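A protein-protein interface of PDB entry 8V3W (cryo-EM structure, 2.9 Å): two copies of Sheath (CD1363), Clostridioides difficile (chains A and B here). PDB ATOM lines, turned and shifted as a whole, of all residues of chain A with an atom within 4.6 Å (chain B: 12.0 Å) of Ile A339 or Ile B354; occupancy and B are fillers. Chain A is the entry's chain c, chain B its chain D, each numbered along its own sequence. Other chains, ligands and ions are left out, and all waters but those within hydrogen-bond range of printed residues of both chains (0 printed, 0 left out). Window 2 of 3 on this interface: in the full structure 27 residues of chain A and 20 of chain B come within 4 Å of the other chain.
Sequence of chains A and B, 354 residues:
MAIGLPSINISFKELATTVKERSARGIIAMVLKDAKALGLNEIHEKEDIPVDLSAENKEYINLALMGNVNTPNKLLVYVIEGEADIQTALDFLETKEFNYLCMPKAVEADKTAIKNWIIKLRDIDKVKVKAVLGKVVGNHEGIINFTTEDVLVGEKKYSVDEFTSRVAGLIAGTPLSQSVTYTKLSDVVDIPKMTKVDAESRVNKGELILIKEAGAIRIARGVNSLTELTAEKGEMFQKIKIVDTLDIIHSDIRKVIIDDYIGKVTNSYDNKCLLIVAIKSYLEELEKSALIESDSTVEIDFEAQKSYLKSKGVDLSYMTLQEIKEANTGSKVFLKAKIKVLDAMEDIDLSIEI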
ATOM      1  N   MET A 236      16.114 -16.241  28.338  1.00  0.00           N
ATOM      2  CA  MET A 236      17.155 -16.029  27.341  1.00  0.00           C
ATOM      3  C   MET A 236      17.271 -14.571  26.926  1.00  0.00           C
ATOM      4  O   MET A 236      18.293 -14.185  26.352  1.00  0.00           O
ATOM      5  CB  MET A 236      16.895 -16.896  26.111  1.00  0.00           C
ATOM      6  CG  MET A 236      15.599 -16.576  25.397  1.00  0.00           C
ATOM      7  SD  MET A 236      15.558 -17.224  23.719  1.00  0.00           S
ATOM      8  CE  MET A 236      15.122 -18.929  24.036  1.00  0.00           C
ATOM      9  N   PHE A 237      16.257 -13.756  27.199  1.00  0.00           N
ATOM     10  CA  PHE A 237      16.293 -12.342  26.855  1.00  0.00           C
ATOM     11  C   PHE A 237      17.033 -11.500  27.881  1.00  0.00           C
ATOM     12  O   PHE A 237      17.149 -10.286  27.693  1.00  0.00           O
ATOM     13  CB  PHE A 237      14.871 -11.810  26.673  1.00  0.00           C
ATOM     14  CG  PHE A 237      14.262 -12.172  25.352  1.00  0.00           C
ATOM     15  CD1 PHE A 237      13.753 -13.437  25.133  1.00  0.00           C
ATOM     16  CD2 PHE A 237      14.209 -11.250  24.325  1.00  0.00           C
ATOM     17  CE1 PHE A 237      13.200 -13.772  23.916  1.00  0.00           C
ATOM     18  CE2 PHE A 237      13.656 -11.582  23.106  1.00  0.00           C
ATOM     19  CZ  PHE A 237      13.150 -12.845  22.903  1.00  0.00           C
ATOM     20  N   LEU A 246      20.172 -11.494  17.947  1.00  0.00           N
ATOM     21  CA  LEU A 246      18.855 -11.305  17.346  1.00  0.00           C
ATOM     22  C   LEU A 246      18.791 -10.006  16.554  1.00  0.00           C
ATOM     23  O   LEU A 246      18.215  -9.962  15.459  1.00  0.00           O
ATOM     24  CB  LEU A 246      17.772 -11.330  18.422  1.00  0.00           C
ATOM     25  CG  LEU A 246      17.512 -12.664  19.121  1.00  0.00           C
ATOM     26  CD1 LEU A 246      16.485 -12.493  20.225  1.00  0.00           C
ATOM     27  CD2 LEU A 246      17.063 -13.715  18.131  1.00  0.00           C
ATOM     28  N   ILE A 249      20.630 -10.414  13.252  1.00  0.00           N
ATOM     29  CA  ILE A 249      19.824 -11.178  12.300  1.00  0.00           C
ATOM     30  C   ILE A 249      18.746 -10.292  11.685  1.00  0.00           C
ATOM     31  O   ILE A 249      18.550 -10.271  10.460  1.00  0.00           O
ATOM     32  CB  ILE A 249      19.211 -12.409  12.991  1.00  0.00           C
ATOM     33  CG1 ILE A 249      20.302 -13.409  13.363  1.00  0.00           C
ATOM     34  CG2 ILE A 249      18.158 -13.050  12.114  1.00  0.00           C
ATOM     35  CD1 ILE A 249      19.811 -14.558  14.193  1.00  0.00           C
ATOM     36  N   LEU A 283      21.144 -17.605   6.416  1.00  0.00           N
ATOM     37  CA  LEU A 283      21.109 -18.357   7.666  1.00  0.00           C
ATOM     38  C   LEU A 283      22.211 -19.409   7.712  1.00  0.00           C
ATOM     39  O   LEU A 283      22.791 -19.662   8.770  1.00  0.00           O
ATOM     40  CB  LEU A 283      19.739 -18.997   7.861  1.00  0.00           C
ATOM     41  CG  LEU A 283      18.658 -18.012   8.303  1.00  0.00           C
ATOM     42  CD1 LEU A 283      17.347 -18.725   8.523  1.00  0.00           C
ATOM     43  CD2 LEU A 283      19.085 -17.276   9.554  1.00  0.00           C
ATOM     44  N   SER A 296      18.429 -25.326  10.325  1.00  0.00           N
ATOM     45  CA  SER A 296      17.460 -24.242  10.273  1.00  0.00           C
ATOM     46  C   SER A 296      16.587 -24.416   9.040  1.00  0.00           C
ATOM     47  O   SER A 296      16.994 -25.032   8.053  1.00  0.00           O
ATOM     48  CB  SER A 296      18.146 -22.874  10.237  1.00  0.00           C
ATOM     49  OG  SER A 296      19.225 -22.818  11.148  1.00  0.00           O
ATOM     50  N   ALA A 337      10.214 -19.297   9.866  1.00  0.00           N
ATOM     51  CA  ALA A 337      11.546 -19.867   9.991  1.00  0.00           C
ATOM     52  C   ALA A 337      11.764 -20.384  11.405  1.00  0.00           C
ATOM     53  O   ALA A 337      11.077 -19.983  12.345  1.00  0.00           O
ATOM     54  CB  ALA A 337      12.627 -18.846   9.625  1.00  0.00           C
ATOM     55  N   LYS A 338      12.736 -21.285  11.542  1.00  0.00           N
ATOM     56  CA  LYS A 338      13.122 -21.853  12.828  1.00  0.00           C
ATOM     57  C   LYS A 338      14.630 -21.756  12.991  1.00  0.00           C
ATOM     58  O   LYS A 338      15.377 -22.218  12.126  1.00  0.00           O
ATOM     59  CB  LYS A 338      12.692 -23.315  12.950  1.00  0.00           C
ATOM     60  CG  LYS A 338      11.212 -23.530  13.144  1.00  0.00           C
ATOM     61  CD  LYS A 338      10.948 -24.865  13.813  1.00  0.00           C
ATOM     62  CE  LYS A 338       9.506 -25.292  13.628  1.00  0.00           C
ATOM     63  NZ  LYS A 338       9.262 -25.814  12.256  1.00  0.00           N
ATOM     64  N   ILE A 339      15.075 -21.170  14.103  1.00  0.00           N
ATOM     65  CA  ILE A 339      16.490 -21.104  14.443  1.00  0.00           C
ATOM     66  C   ILE A 339      16.656 -21.417  15.922  1.00  0.00           C
ATOM     67  O   ILE A 339      15.701 -21.384  16.699  1.00  0.00           O
ATOM     68  CB  ILE A 339      17.125 -19.731  14.130  1.00  0.00           C
ATOM     69  CG1 ILE A 339      16.528 -18.648  15.025  1.00  0.00           C
ATOM     70  CG2 ILE A 339      16.960 -19.372  12.669  1.00  0.00           C
ATOM     71  CD1 ILE A 339      17.211 -17.313  14.902  1.00  0.00           C
ATOM     72  N   LYS A 340      17.891 -21.728  16.302  1.00  0.00           N
ATOM     73  CA  LYS A 340      18.267 -21.877  17.701  1.00  0.00           C
ATOM     74  C   LYS A 340      19.583 -21.150  17.922  1.00  0.00           C
ATOM     75  O   LYS A 340      20.543 -21.370  17.181  1.00  0.00           O
ATOM     76  CB  LYS A 340      18.391 -23.350  18.094  1.00  0.00           C
ATOM     77  CG  LYS A 340      18.687 -23.566  19.565  1.00  0.00           C
ATOM     78  CD  LYS A 340      17.550 -23.063  20.432  1.00  0.00           C
ATOM     79  CE  LYS A 340      17.775 -23.415  21.891  1.00  0.00           C
ATOM     80  NZ  LYS A 340      16.525 -23.301  22.689  1.00  0.00           N
ATOM     81  N   VAL A 341      19.627 -20.295  18.940  1.00  0.00           N
ATOM     82  CA  VAL A 341      20.748 -19.389  19.164  1.00  0.00           C
ATOM     83  C   VAL A 341      21.644 -19.957  20.253  1.00  0.00           C
ATOM     84  O   VAL A 341      21.164 -20.350  21.323  1.00  0.00           O
ATOM     85  CB  VAL A 341      20.259 -17.981  19.536  1.00  0.00           C
ATOM     86  CG1 VAL A 341      21.435 -17.081  19.851  1.00  0.00           C
ATOM     87  CG2 VAL A 341      19.431 -17.395  18.413  1.00  0.00           C
ATOM     88  N   LEU B 350       7.812 -12.107   8.142  1.00  0.00           N
ATOM     89  CA  LEU B 350       8.712 -13.217   8.441  1.00  0.00           C
ATOM     90  C   LEU B 350       8.658 -13.497   9.935  1.00  0.00           C
ATOM     91  O   LEU B 350       9.228 -12.746  10.730  1.00  0.00           O
ATOM     92  CB  LEU B 350      10.141 -12.905   7.997  1.00  0.00           C
ATOM     93  CG  LEU B 350      11.201 -13.973   8.273  1.00  0.00           C
ATOM     94  CD1 LEU B 350      10.724 -15.346   7.854  1.00  0.00           C
ATOM     95  CD2 LEU B 350      12.499 -13.631   7.580  1.00  0.00           C
ATOM     96  N   SER B 351       7.989 -14.581  10.311  1.00  0.00           N
ATOM     97  CA  SER B 351       7.852 -14.983  11.704  1.00  0.00           C
ATOM     98  C   SER B 351       8.906 -16.035  12.023  1.00  0.00           C
ATOM     99  O   SER B 351       8.966 -17.074  11.363  1.00  0.00           O
ATOM    100  CB  SER B 351       6.450 -15.526  11.973  1.00  0.00           C
ATOM    101  OG  SER B 351       6.214 -15.654  13.361  1.00  0.00           O
ATOM    102  N   ILE B 352       9.725 -15.771  13.035  1.00  0.00           N
ATOM    103  CA  ILE B 352      10.861 -16.620  13.373  1.00  0.00           C
ATOM    104  C   ILE B 352      10.658 -17.181  14.772  1.00  0.00           C
ATOM    105  O   ILE B 352      10.371 -16.430  15.710  1.00  0.00           O
ATOM    106  CB  ILE B 352      12.187 -15.847  13.281  1.00  0.00           C
ATOM    107  CG1 ILE B 352      12.313 -15.186  11.910  1.00  0.00           C
ATOM    108  CG2 ILE B 352      13.361 -16.762  13.546  1.00  0.00           C
ATOM    109  CD1 ILE B 352      13.607 -14.465  11.699  1.00  0.00           C
ATOM    110  N   GLU B 353      10.809 -18.494  14.910  1.00  0.00           N
ATOM    111  CA  GLU B 353      10.723 -19.171  16.196  1.00  0.00           C
ATOM    112  C   GLU B 353      12.131 -19.472  16.686  1.00  0.00           C
ATOM    113  O   GLU B 353      12.917 -20.103  15.975  1.00  0.00           O
ATOM    114  CB  GLU B 353       9.912 -20.460  16.091  1.00  0.00           C
ATOM    115  CG  GLU B 353       8.534 -20.287  15.498  1.00  0.00           C
ATOM    116  CD  GLU B 353       7.705 -21.552  15.589  1.00  0.00           C
ATOM    117  OE1 GLU B 353       7.483 -22.035  16.716  1.00  0.00           O
ATOM    118  OE2 GLU B 353       7.278 -22.065  14.534  1.00  0.00           O
ATOM    119  N   ILE B 354      12.441 -19.027  17.897  1.00  0.00           N
ATOM    120  CA  ILE B 354      13.764 -19.221  18.461  1.00  0.00           C
ATOM    121  C   ILE B 354      13.734 -20.312  19.521  1.00  0.00           C
ATOM    122  O   ILE B 354      13.744 -21.500  19.200  1.00  0.00           O
ATOM    123  CB  ILE B 354      14.308 -17.911  19.038  1.00  0.00           C
ATOM    124  CG1 ILE B 354      13.262 -17.253  19.936  1.00  0.00           C
ATOM    125  CG2 ILE B 354      14.711 -16.971  17.923  1.00  0.00           C
ATOM    126  CD1 ILE B 354      13.792 -16.089  20.724  1.00  0.00           C
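The backbone NH (N) of Ala A337 is in hydrogen-bond range of the backbone carbonyl oxygen (O) of Ser B351 (3.0 Å).
The backbone carbonyl oxygen (O) of Ala A337 lies within hydrogen-bond range of the backbone NH (N) of Glu B353, 3.0 Å away.
N of Ile A339 lies within hydrogen-bond range of O of Glu B353, 3.0 Å away.
O of Ile A339 lies close to O of Ile B354.
Printed residues of chain B that touch a printed residue of chain A: Ser B351, Ile B352, Glu B353 and Ile B354.
Hydrophobic or aromatic side chains of chain B that line the printed part of chain A: Ile B352 and Ile B354.
Among the printed residues, no Asp or Glu carboxylate lies within 4 Å of a Lys or Arg side-chain nitrogen of the other chain.
Among the printed residues, pairs that only touch across the chains: Ala A337 with Ile B352, Lys A338 with Glu B353, Met A236 with Ile B354, Phe A237 with Ile B354 and Ile A339 with Ile B352.
No position is printed for both chains.
Ile B354 touches just these residues of chain A: Met A236, Phe A237 and Ile A339.
No residue of chain B comes within 4 Å of Leu A246.
No residue of chain B comes within 4 Å of Leu A283.
No residue of chain B comes within 4 Å of Ser A296.
Printed residues of chain B within 4 Å of Ala A337: Ser B351 (3.0 Å), Ile B352 (3.5 Å) and Glu B353 (3.0 Å).
Lys A338 touches one residue of chain B.
Val A341 touches none of the printed residues of chain B.
Of the printed residues of chain B, Met A236 touches Ile B354 (3.7 Å).
Of the printed residues of chain A, Ser B351 touches Ala A337 (3.0 Å).
Printed residues of chain A within 4 Å of Ile B352: Ala A337 (3.5 Å) and Ile A339 (3.97 Å).
Printed residues of chain A within 4 Å of Glu B353: Ala A337 (3.0 Å), Lys A338 (3.6 Å) and Ile A339 (3.0 Å).
Leu B350 touches none of the printed residues of chain A.
Ile A249 touches none of the printed residues of chain B.
The nearest printed residue of chain A that does not touch Ser B351 is Lys A338 (5.7 Å).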
